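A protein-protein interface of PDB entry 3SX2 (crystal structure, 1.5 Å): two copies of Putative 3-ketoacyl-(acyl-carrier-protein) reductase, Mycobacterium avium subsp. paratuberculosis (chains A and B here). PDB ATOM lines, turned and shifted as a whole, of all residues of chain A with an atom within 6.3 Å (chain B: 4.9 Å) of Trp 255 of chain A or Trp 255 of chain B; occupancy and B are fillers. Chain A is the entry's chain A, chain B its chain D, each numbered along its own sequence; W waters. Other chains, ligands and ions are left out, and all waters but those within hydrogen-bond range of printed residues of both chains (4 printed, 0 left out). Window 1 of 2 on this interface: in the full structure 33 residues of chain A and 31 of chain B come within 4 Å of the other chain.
Asn 251 of chain A touches Gln 260 of chain B, and with the chains exchanged Gln 260 of chain A touches Asn 251 of chain B.
Ala 252 of chain A touches Trp 255 of chain B, and with the chains exchanged Trp 255 of chain A touches Ala 252 of chain B.
Trp 255 of chain A touches its own counterpart, Trp 255 of chain B.
Leu 269 of chain A touches Trp 255 of chain B, but with the chains exchanged Trp 255 of chain A does not touch Leu 269 of chain B (4.04 Å).
Positions printed for both chains: 251, 252, 253, 254, 255, 256, 257, 258, 260, 261, 264 and 269.
Of the 9 pairs that touch across the chains among the printed residues, 5 have their exchanged pair printed and touching as well.
Water W4 lies within hydrogen-bond range of NE2 of Gln 260 of chain B (2.6 Å), O of Asn 251 of chain A (2.7 Å) and NH2 of Arg 32 of chain A (3.5 Å).
Water W1 bridges the side-chain amide nitrogen (NE2) of Gln 260 of chain A (2.7 Å) and the backbone carbonyl oxygen (O) of Asn 251 of chain B (2.7 Å).
Water W3 bridges the side-chain amide nitrogen of Asn 251 of chain A (2.9 Å) and the backbone carbonyl oxygen of Gln 260 of chain B (3.4 Å).
Water W2 lies within hydrogen-bond range of ND2 of Asn 251 of chain B (3.0 Å), O of Asp 259 of chain A (3.1 Å) and O of Gln 260 of chain A (3.5 Å).
The guanidinium group (NH2) of Arg 32 of chain A sits close to the side-chain amide nitrogen (NE2) of Gln 260 of chain B (3.1 Å).
NE2 of Gln 260 of chain A sits close to OD1 of Asn 251 of chain B.
The side-chain amide oxygen (OD1) of Asn 251 of chain A lies close to the side-chain amide nitrogen (NE2) of Gln 260 of chain B, 3.4 Å away.
Of the 21 printed residues of chain A, 8 touch a printed residue of chain B.
Hydrophobic or aromatic side chains of chain A that line the printed part of chain B: Ala 252, Trp 255, Leu 269 and Val 271.
Of the printed residues of chain B, Arg 32 of chain A touches Gln 260.
Leu 33 of chain A touches none of the printed residues of chain B.
Of the printed residues of chain B, Ala 252 of chain A touches Trp 255 (3.9 Å).
Of the printed residues of chain B, Trp 255 of chain A touches Ala 252 (3.9 Å) and Trp 255 (3.5 Å).
Printed residues of chain A within 4 Å of Trp 255 of chain B: Ala 252 (3.9 Å), Trp 255 (3.5 Å) and Leu 269 (3.9 Å).
Of the printed residues of chain A, Gln 260 of chain B touches Arg 32 and Asn 251.
Ala 261 of chain B touches none of the printed residues of chain A.
The nearest printed residue of chain B that does not touch Trp 255 of chain A is Leu 269 of chain B (4.04 Å).
The nearest printed residue of chain A that does not touch Trp 255 of chain B is Asn 251 of chain A (4.2 Å).
The nearest printed residue of chain A that does not touch Ala 252 of chain B is Gln 260 of chain A (4.3 Å).
The side-chain hydroxyl of Ser 258 of chain B is in hydrogen-bond range of the backbone carbonyl oxygen of Trp 255 of chain B (2.7 Å).
N of Gln 260 of chain B sits close to OG of Ser 258 of chain B (3.2 Å).
OD1 of Asn 251 of chain A lies within hydrogen-bond range of NE of Arg 32 of chain A (2.9 Å).
The side-chain hydroxyl (OG) of Ser 258 of chain A lies close to the backbone NH (N) of Gln 260 of chain A, at 3.2 Å.
O of Trp 255 of chain A is in hydrogen-bond range of OG of Ser 258 of chain A.
The guanidinium group (NH1) of Arg 32 of chain A lies within salt-bridge range of the side-chain carboxylate (OD2) of Asp 36 of chain A (2.7 Å).
Among the printed residues, merely in contact across the chains: Val 271 of chain A with Ile 264 of chain B (3.5 Å), Trp 255 of chain A with Trp 255 of chain B (3.5 Å), Pro 270 of chain A with Ile 264 of chain B (3.8 Å), Ala 252 of chain A with Trp 255 of chain B (3.9 Å), Leu 269 of chain A with Trp 255 of chain B (3.9 Å) and Trp 255 of chain A with Ala 252 of chain B (3.9 Å).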
ATOM      1  N   ARG A  32      19.226  24.972 -29.182  1.00  0.00           N
ATOM      2  CA  ARG A  32      18.704  24.599 -27.867  1.00  0.00           C
ATOM      3  C   ARG A  32      19.615  23.610 -27.143  1.00  0.00           C
ATOM      4  O   ARG A  32      19.877  23.743 -25.936  1.00  0.00           O
ATOM      5  CB  ARG A  32      17.286  24.052 -27.974  1.00  0.00           C
ATOM      6  CG  ARG A  32      16.689  23.624 -26.625  1.00  0.00           C
ATOM      7  CD  ARG A  32      16.395  24.836 -25.741  1.00  0.00           C
ATOM      8  NE  ARG A  32      15.684  24.489 -24.513  1.00  0.00           N
ATOM      9  CZ  ARG A  32      16.319  23.946 -23.498  1.00  0.00           C
ATOM     10  NH1 ARG A  32      17.600  23.744 -23.620  1.00  0.00           N
ATOM     11  NH2 ARG A  32      15.711  23.606 -22.374  1.00  0.00           N
ATOM     12  N   LEU A  33      20.071  22.589 -27.847  1.00  0.00           N
ATOM     13  CA  LEU A  33      20.906  21.592 -27.201  1.00  0.00           C
ATOM     14  C   LEU A  33      22.300  22.183 -26.937  1.00  0.00           C
ATOM     15  O   LEU A  33      22.911  21.875 -25.922  1.00  0.00           O
ATOM     16  CB  LEU A  33      20.971  20.333 -28.068  1.00  0.00           C
ATOM     17  CG  LEU A  33      19.623  19.611 -28.282  1.00  0.00           C
ATOM     18  CD1 LEU A  33      19.801  18.404 -29.242  1.00  0.00           C
ATOM     19  CD2 LEU A  33      19.001  19.154 -26.996  1.00  0.00           C
ATOM     20  N   ASP A  36      22.257  24.079 -23.721  1.00  0.00           N
ATOM     21  CA  ASP A  36      22.370  23.167 -22.577  1.00  0.00           C
ATOM     22  C   ASP A  36      23.741  22.516 -22.438  1.00  0.00           C
ATOM     23  O   ASP A  36      23.944  21.683 -21.550  1.00  0.00           O
ATOM     24  CB  ASP A  36      21.300  22.065 -22.692  1.00  0.00           C
ATOM     25  CG  ASP A  36      19.929  22.513 -22.158  1.00  0.00           C
ATOM     26  OD1 ASP A  36      19.821  23.641 -21.621  1.00  0.00           O
ATOM     27  OD2 ASP A  36      18.938  21.751 -22.289  1.00  0.00           O
ATOM     28  N   ARG A 199      17.273   5.283 -25.311  1.00  0.00           N
ATOM     29  CA  ARG A 199      15.870   5.652 -25.420  1.00  0.00           C
ATOM     30  C   ARG A 199      15.540   6.032 -26.860  1.00  0.00           C
ATOM     31  O   ARG A 199      16.359   6.641 -27.547  1.00  0.00           O
ATOM     32  CB  ARG A 199      15.541   6.815 -24.494  1.00  0.00           C
ATOM     33  CG  ARG A 199      15.803   6.507 -23.025  1.00  0.00           C
ATOM     34  CD  ARG A 199      17.042   7.230 -22.505  1.00  0.00           C
ATOM     35  NE  ARG A 199      16.766   8.646 -22.312  1.00  0.00           N
ATOM     36  CZ  ARG A 199      17.597   9.520 -21.760  1.00  0.00           C
ATOM     37  NH1 ARG A 199      18.768   9.131 -21.315  1.00  0.00           N
ATOM     38  NH2 ARG A 199      17.217  10.782 -21.627  1.00  0.00           N
ATOM     39  N   ALA A 250      11.849  22.083 -29.994  1.00  0.00           N
ATOM     40  CA  ALA A 250      13.179  21.956 -29.447  1.00  0.00           C
ATOM     41  C   ALA A 250      13.156  21.847 -27.949  1.00  0.00           C
ATOM     42  O   ALA A 250      13.945  21.101 -27.363  1.00  0.00           O
ATOM     43  CB  ALA A 250      14.058  23.135 -29.928  1.00  0.00           C
ATOM     44  N   ASN A 251      12.207  22.521 -27.298  1.00  0.00           N
ATOM     45  CA  ASN A 251      12.116  22.441 -25.829  1.00  0.00           C
ATOM     46  C   ASN A 251      11.685  21.049 -25.392  1.00  0.00           C
ATOM     47  O   ASN A 251      12.222  20.502 -24.386  1.00  0.00           O
ATOM     48  CB  ASN A 251      11.173  23.518 -25.307  1.00  0.00           C
ATOM     49  CG  ASN A 251      11.788  24.916 -25.394  1.00  0.00           C
ATOM     50  OD1 ASN A 251      12.999  25.053 -25.596  1.00  0.00           O
ATOM     51  ND2 ASN A 251      10.956  25.966 -25.262  1.00  0.00           N
ATOM     52  N   ALA A 252      10.739  20.428 -26.098  1.00  0.00           N
ATOM     53  CA  ALA A 252      10.323  19.061 -25.783  1.00  0.00           C
ATOM     54  C   ALA A 252      11.479  18.073 -25.918  1.00  0.00           C
ATOM     55  O   ALA A 252      11.707  17.230 -25.031  1.00  0.00           O
ATOM     56  CB  ALA A 252       9.139  18.662 -26.679  1.00  0.00           C
ATOM     57  N   VAL A 253      12.232  18.181 -27.000  1.00  0.00           N
ATOM     58  CA  VAL A 253      13.376  17.325 -27.252  1.00  0.00           C
ATOM     59  C   VAL A 253      14.469  17.541 -26.211  1.00  0.00           C
ATOM     60  O   VAL A 253      15.077  16.554 -25.732  1.00  0.00           O
ATOM     61  CB  VAL A 253      13.882  17.506 -28.694  1.00  0.00           C
ATOM     62  CG1 VAL A 253      15.196  16.826 -28.932  1.00  0.00           C
ATOM     63  CG2 VAL A 253      12.784  16.981 -29.690  1.00  0.00           C
ATOM     64  N   ALA A 254      14.730  18.789 -25.820  1.00  0.00           N
ATOM     65  CA  ALA A 254      15.750  19.059 -24.806  1.00  0.00           C
ATOM     66  C   ALA A 254      15.414  18.409 -23.488  1.00  0.00           C
ATOM     67  O   ALA A 254      16.315  17.927 -22.773  1.00  0.00           O
ATOM     68  CB  ALA A 254      15.875  20.565 -24.573  1.00  0.00           C
ATOM     69  N   TRP A 255      14.132  18.344 -23.139  1.00  0.00           N
ATOM     70  CA  TRP A 255      13.670  17.604 -21.932  1.00  0.00           C
ATOM     71  C   TRP A 255      13.935  16.116 -22.110  1.00  0.00           C
ATOM     72  O   TRP A 255      14.545  15.424 -21.249  1.00  0.00           O
ATOM     73  CB  TRP A 255      12.153  17.793 -21.639  1.00  0.00           C
ATOM     74  CG  TRP A 255      11.604  16.795 -20.596  1.00  0.00           C
ATOM     75  CD1 TRP A 255      11.951  16.701 -19.268  1.00  0.00           C
ATOM     76  CD2 TRP A 255      10.652  15.754 -20.828  1.00  0.00           C
ATOM     77  NE1 TRP A 255      11.266  15.665 -18.674  1.00  0.00           N
ATOM     78  CE2 TRP A 255      10.472  15.065 -19.615  1.00  0.00           C
ATOM     79  CE3 TRP A 255       9.948  15.319 -21.957  1.00  0.00           C
ATOM     80  CZ2 TRP A 255       9.611  13.970 -19.504  1.00  0.00           C
ATOM     81  CZ3 TRP A 255       9.096  14.253 -21.840  1.00  0.00           C
ATOM     82  CH2 TRP A 255       8.940  13.580 -20.635  1.00  0.00           C
ATOM     83  N   LEU A 256      13.466  15.550 -23.217  1.00  0.00           N
ATOM     84  CA  LEU A 256      13.496  14.117 -23.451  1.00  0.00           C
ATOM     85  C   LEU A 256      14.881  13.530 -23.362  1.00  0.00           C
ATOM     86  O   LEU A 256      15.084  12.433 -22.834  1.00  0.00           O
ATOM     87  CB  LEU A 256      12.942  13.766 -24.839  1.00  0.00           C
ATOM     88  CG  LEU A 256      11.520  13.311 -25.039  1.00  0.00           C
ATOM     89  CD1 LEU A 256      11.374  12.993 -26.519  1.00  0.00           C
ATOM     90  CD2 LEU A 256      11.100  12.145 -24.119  1.00  0.00           C
ATOM     91  N   VAL A 257      15.886  14.299 -23.849  1.00  0.00           N
ATOM     92  CA  VAL A 257      17.239  13.787 -23.933  1.00  0.00           C
ATOM     93  C   VAL A 257      18.058  14.035 -22.633  1.00  0.00           C
ATOM     94  O   VAL A 257      19.213  13.591 -22.488  1.00  0.00           O
ATOM     95  CB  VAL A 257      17.994  14.324 -25.146  1.00  0.00           C
ATOM     96  CG1 VAL A 257      17.201  14.031 -26.415  1.00  0.00           C
ATOM     97  CG2 VAL A 257      18.328  15.843 -25.018  1.00  0.00           C
ATOM     98  N   SER A 258      17.417  14.690 -21.672  1.00  0.00           N
ATOM     99  CA  SER A 258      18.034  14.983 -20.385  1.00  0.00           C
ATOM    100  C   SER A 258      17.822  13.863 -19.377  1.00  0.00           C
ATOM    101  O   SER A 258      16.960  13.005 -19.568  1.00  0.00           O
ATOM    102  CB  SER A 258      17.456  16.271 -19.798  1.00  0.00           C
ATOM    103  OG  SER A 258      16.181  16.119 -19.231  1.00  0.00           O
ATOM    104  N   ASP A 259      18.544  13.930 -18.255  1.00  0.00           N
ATOM    105  CA  ASP A 259      18.338  12.964 -17.168  1.00  0.00           C
ATOM    106  C   ASP A 259      16.973  13.058 -16.526  1.00  0.00           C
ATOM    107  O   ASP A 259      16.530  12.107 -15.871  1.00  0.00           O
ATOM    108  CB  ASP A 259      19.456  13.114 -16.108  1.00  0.00           C
ATOM    109  CG  ASP A 259      20.800  12.570 -16.584  1.00  0.00           C
ATOM    110  OD1 ASP A 259      20.833  11.756 -17.538  1.00  0.00           O
ATOM    111  OD2 ASP A 259      21.843  12.915 -15.949  1.00  0.00           O
ATOM    112  N   GLN A 260      16.268  14.174 -16.717  1.00  0.00           N
ATOM    113  CA  GLN A 260      14.897  14.351 -16.225  1.00  0.00           C
ATOM    114  C   GLN A 260      13.880  13.443 -16.956  1.00  0.00           C
ATOM    115  O   GLN A 260      12.651  13.427 -16.617  1.00  0.00           O
ATOM    116  CB  GLN A 260      14.420  15.800 -16.413  1.00  0.00           C
ATOM    117  CG  GLN A 260      15.295  16.881 -15.719  1.00  0.00           C
ATOM    118  CD  GLN A 260      15.098  16.878 -14.245  1.00  0.00           C
ATOM    119  OE1 GLN A 260      16.014  16.556 -13.467  1.00  0.00           O
ATOM    120  NE2 GLN A 260      13.899  17.204 -13.824  1.00  0.00           N
ATOM    121  N   ALA A 261      14.337  12.823 -18.051  1.00  0.00           N
ATOM    122  CA  ALA A 261      13.506  11.908 -18.831  1.00  0.00           C
ATOM    123  C   ALA A 261      14.271  10.605 -19.091  1.00  0.00           C
ATOM    124  O   ALA A 261      14.080   9.931 -20.109  1.00  0.00           O
ATOM    125  CB  ALA A 261      13.098  12.568 -20.167  1.00  0.00           C
ATOM    126  N   ARG A 262      15.073  10.198 -18.134  1.00  0.00           N
ATOM    127  CA  ARG A 262      16.041   9.098 -18.316  1.00  0.00           C
ATOM    128  C   ARG A 262      15.369   7.775 -18.641  1.00  0.00           C
ATOM    129  O   ARG A 262      16.001   6.905 -19.272  1.00  0.00           O
ATOM    130  CB  ARG A 262      16.926   8.904 -17.063  1.00  0.00           C
ATOM    131  CG  ARG A 262      16.152   8.667 -15.766  1.00  0.00           C
ATOM    132  CD  ARG A 262      17.061   8.545 -14.530  1.00  0.00           C
ATOM    133  NE  ARG A 262      16.264   8.239 -13.376  1.00  0.00           N
ATOM    134  CZ  ARG A 262      16.740   7.842 -12.199  1.00  0.00           C
ATOM    135  NH1 ARG A 262      18.056   7.730 -12.016  1.00  0.00           N
ATOM    136  NH2 ARG A 262      15.903   7.511 -11.248  1.00  0.00           N
ATOM    137  N   ILE A 264      12.176   7.465 -20.129  1.00  0.00           N
ATOM    138  CA  ILE A 264      11.124   7.661 -21.131  1.00  0.00           C
ATOM    139  C   ILE A 264      11.551   7.007 -22.450  1.00  0.00           C
ATOM    140  O   ILE A 264      12.493   7.488 -23.107  1.00  0.00           O
ATOM    141  CB  ILE A 264      10.801   9.168 -21.336  1.00  0.00           C
ATOM    142  CG1 ILE A 264      10.619   9.878 -19.988  1.00  0.00           C
ATOM    143  CG2 ILE A 264       9.599   9.345 -22.235  1.00  0.00           C
ATOM    144  CD1 ILE A 264       9.459   9.344 -19.188  1.00  0.00           C
ATOM    145  N   LEU A 269       5.048  11.319 -28.678  1.00  0.00           N
ATOM    146  CA  LEU A 269       4.740  12.538 -27.919  1.00  0.00           C
ATOM    147  C   LEU A 269       4.194  13.650 -28.836  1.00  0.00           C
ATOM    148  O   LEU A 269       4.985  14.292 -29.542  1.00  0.00           O
ATOM    149  CB  LEU A 269       6.026  13.063 -27.242  1.00  0.00           C
ATOM    150  CG  LEU A 269       5.891  14.334 -26.398  1.00  0.00           C
ATOM    151  CD1 LEU A 269       4.849  14.185 -25.304  1.00  0.00           C
ATOM    152  CD2 LEU A 269       7.276  14.770 -25.822  1.00  0.00           C
ATOM    153  N   PRO A 270       2.889  13.930 -28.775  1.00  0.00           N
ATOM    154  CA  PRO A 270       2.336  15.080 -29.499  1.00  0.00           C
ATOM    155  C   PRO A 270       2.791  16.399 -28.859  1.00  0.00           C
ATOM    156  O   PRO A 270       2.768  16.533 -27.635  1.00  0.00           O
ATOM    157  CB  PRO A 270       0.841  14.901 -29.355  1.00  0.00           C
ATOM    158  CG  PRO A 270       0.637  13.429 -29.053  1.00  0.00           C
ATOM    159  CD  PRO A 270       1.807  13.138 -28.173  1.00  0.00           C
ATOM    160  N   VAL A 271       3.261  17.308 -29.697  1.00  0.00           N
ATOM    161  CA  VAL A 271       3.584  18.672 -29.293  1.00  0.00           C
ATOM    162  C   VAL A 271       2.747  19.539 -30.210  1.00  0.00           C
ATOM    163  O   VAL A 271       3.178  19.893 -31.315  1.00  0.00           O
ATOM    164  CB  VAL A 271       5.091  18.954 -29.423  1.00  0.00           C
ATOM    165  CG1 VAL A 271       5.404  20.383 -29.004  1.00  0.00           C
ATOM    166  CG2 VAL A 271       5.893  17.970 -28.575  1.00  0.00           C
ATOM    167  N   ASN B 251       9.657  14.497 -12.039  1.00  0.00           N
ATOM    168  CA  ASN B 251      10.456  15.229 -13.040  1.00  0.00           C
ATOM    169  C   ASN B 251       9.653  15.413 -14.297  1.00  0.00           C
ATOM    170  O   ASN B 251       9.670  16.477 -14.927  1.00  0.00           O
ATOM    171  CB  ASN B 251      11.766  14.511 -13.317  1.00  0.00           C
ATOM    172  CG  ASN B 251      12.762  14.648 -12.182  1.00  0.00           C
ATOM    173  OD1 ASN B 251      12.606  15.488 -11.286  1.00  0.00           O
ATOM    174  ND2 ASN B 251      13.798  13.817 -12.214  1.00  0.00           N
ATOM    175  N   ALA B 252       8.921  14.378 -14.724  1.00  0.00           N
ATOM    176  CA  ALA B 252       8.070  14.531 -15.924  1.00  0.00           C
ATOM    177  C   ALA B 252       7.004  15.599 -15.697  1.00  0.00           C
ATOM    178  O   ALA B 252       6.777  16.446 -16.568  1.00  0.00           O
ATOM    179  CB  ALA B 252       7.433  13.185 -16.318  1.00  0.00           C
ATOM    180  N   VAL B 253       6.357  15.569 -14.543  1.00  0.00           N
ATOM    181  CA  VAL B 253       5.297  16.548 -14.234  1.00  0.00           C
ATOM    182  C   VAL B 253       5.855  17.984 -14.169  1.00  0.00           C
ATOM    183  O   VAL B 253       5.226  18.900 -14.675  1.00  0.00           O
ATOM    184  CB  VAL B 253       4.579  16.136 -12.975  1.00  0.00           C
ATOM    185  CG1 VAL B 253       3.692  17.255 -12.446  1.00  0.00           C
ATOM    186  CG2 VAL B 253       3.739  14.900 -13.300  1.00  0.00           C
ATOM    187  N   ALA B 254       7.019  18.164 -13.568  1.00  0.00           N
ATOM    188  CA  ALA B 254       7.655  19.473 -13.468  1.00  0.00           C
ATOM    189  C   ALA B 254       7.890  20.046 -14.842  1.00  0.00           C
ATOM    190  O   ALA B 254       7.691  21.248 -15.039  1.00  0.00           O
ATOM    191  CB  ALA B 254       8.996  19.354 -12.652  1.00  0.00           C
ATOM    192  N   TRP B 255       8.293  19.212 -15.790  1.00  0.00           N
ATOM    193  CA  TRP B 255       8.480  19.645 -17.201  1.00  0.00           C
ATOM    194  C   TRP B 255       7.171  20.111 -17.771  1.00  0.00           C
ATOM    195  O   TRP B 255       7.023  21.232 -18.310  1.00  0.00           O
ATOM    196  CB  TRP B 255       8.988  18.511 -18.125  1.00  0.00           C
ATOM    197  CG  TRP B 255       8.889  18.869 -19.632  1.00  0.00           C
ATOM    198  CD1 TRP B 255       9.524  19.896 -20.291  1.00  0.00           C
ATOM    199  CD2 TRP B 255       8.082  18.212 -20.621  1.00  0.00           C
ATOM    200  NE1 TRP B 255       9.179  19.886 -21.611  1.00  0.00           N
ATOM    201  CE2 TRP B 255       8.277  18.881 -21.835  1.00  0.00           C
ATOM    202  CE3 TRP B 255       7.201  17.128 -20.594  1.00  0.00           C
ATOM    203  CZ2 TRP B 255       7.634  18.485 -23.014  1.00  0.00           C
ATOM    204  CZ3 TRP B 255       6.579  16.736 -21.751  1.00  0.00           C
ATOM    205  CH2 TRP B 255       6.787  17.406 -22.940  1.00  0.00           C
ATOM    206  N   LEU B 256       6.184  19.243 -17.673  1.00  0.00           N
ATOM    207  CA  LEU B 256       4.868  19.452 -18.296  1.00  0.00           C
ATOM    208  C   LEU B 256       4.167  20.720 -17.862  1.00  0.00           C
ATOM    209  O   LEU B 256       3.524  21.394 -18.688  1.00  0.00           O
ATOM    210  CB  LEU B 256       3.992  18.252 -17.976  1.00  0.00           C
ATOM    211  CG  LEU B 256       2.943  17.711 -18.863  1.00  0.00           C
ATOM    212  CD1 LEU B 256       3.399  17.598 -20.369  1.00  0.00           C
ATOM    213  CD2 LEU B 256       2.511  16.356 -18.297  1.00  0.00           C
ATOM    214  N   VAL B 257       4.327  21.091 -16.594  1.00  0.00           N
ATOM    215  CA  VAL B 257       3.639  22.266 -16.071  1.00  0.00           C
ATOM    216  C   VAL B 257       4.449  23.551 -16.302  1.00  0.00           C
ATOM    217  O   VAL B 257       3.981  24.639 -15.930  1.00  0.00           O
ATOM    218  CB  VAL B 257       3.246  22.081 -14.590  1.00  0.00           C
ATOM    219  CG1 VAL B 257       2.394  20.818 -14.442  1.00  0.00           C
ATOM    220  CG2 VAL B 257       4.474  22.054 -13.640  1.00  0.00           C
ATOM    221  N   SER B 258       5.636  23.444 -16.884  1.00  0.00           N
ATOM    222  CA  SER B 258       6.532  24.578 -17.117  1.00  0.00           C
ATOM    223  C   SER B 258       6.218  25.213 -18.480  1.00  0.00           C
ATOM    224  O   SER B 258       5.529  24.622 -19.310  1.00  0.00           O
ATOM    225  CB  SER B 258       8.013  24.140 -17.095  1.00  0.00           C
ATOM    226  OG  SER B 258       8.416  23.515 -18.304  1.00  0.00           O
ATOM    227  N   GLN B 260       8.235  25.418 -20.871  1.00  0.00           N
ATOM    228  CA  GLN B 260       8.866  24.536 -21.854  1.00  0.00           C
ATOM    229  C   GLN B 260       7.877  23.515 -22.473  1.00  0.00           C
ATOM    230  O   GLN B 260       8.240  22.757 -23.424  1.00  0.00           O
ATOM    231  CB  GLN B 260       9.991  23.744 -21.210  1.00  0.00           C
ATOM    232  CG  GLN B 260      11.098  24.558 -20.586  1.00  0.00           C
ATOM    233  CD  GLN B 260      11.986  25.165 -21.612  1.00  0.00           C
ATOM    234  OE1 GLN B 260      12.071  26.377 -21.750  1.00  0.00           O
ATOM    235  NE2 GLN B 260      12.706  24.329 -22.302  1.00  0.00           N
ATOM    236  N   ALA B 261       6.698  23.381 -21.861  1.00  0.00           N
ATOM    237  CA  ALA B 261       5.660  22.485 -22.363  1.00  0.00           C
ATOM    238  C   ALA B 261       4.317  23.242 -22.467  1.00  0.00           C
ATOM    239  O   ALA B 261       3.232  22.650 -22.330  1.00  0.00           O
ATOM    240  CB  ALA B 261       5.518  21.243 -21.411  1.00  0.00           C
ATOM    241  N   ILE B 264       1.511  21.642 -24.740  1.00  0.00           N
ATOM    242  CA  ILE B 264       1.299  20.197 -24.653  1.00  0.00           C
ATOM    243  C   ILE B 264      -0.034  19.948 -23.930  1.00  0.00           C
ATOM    244  O   ILE B 264      -0.157  20.258 -22.729  1.00  0.00           O
ATOM    245  CB  ILE B 264       2.457  19.519 -23.886  1.00  0.00           C
ATOM    246  CG1 ILE B 264       3.833  20.015 -24.395  1.00  0.00           C
ATOM    247  CG2 ILE B 264       2.339  17.999 -23.965  1.00  0.00           C
ATOM    248  CD1 ILE B 264       4.149  19.600 -25.828  1.00  0.00           C
ATOM    249  N   LEU B 269       1.032  10.345 -21.399  1.00  0.00           N
ATOM    250  CA  LEU B 269       2.497  10.266 -21.354  1.00  0.00           C
ATOM    251  C   LEU B 269       2.972   9.068 -20.476  1.00  0.00           C
ATOM    252  O   LEU B 269       2.935   9.137 -19.240  1.00  0.00           O
ATOM    253  CB  LEU B 269       3.082  11.580 -20.821  1.00  0.00           C
ATOM    254  CG  LEU B 269       4.597  11.618 -20.659  1.00  0.00           C
ATOM    255  CD1 LEU B 269       5.332  11.359 -21.969  1.00  0.00           C
ATOM    256  CD2 LEU B 269       4.996  12.970 -19.987  1.00  0.00           C
HETATM  257  O   HOH W   1      11.861  18.033 -15.397  1.00  0.00           O
HETATM  258  O   HOH W   2      14.091  11.524 -14.064  1.00  0.00           O
HETATM  259  O   HOH W   3       8.050  25.623 -25.212  1.00  0.00           O
HETATM  260  O   HOH W   4      12.794  21.727 -22.024  1.00  0.00           O
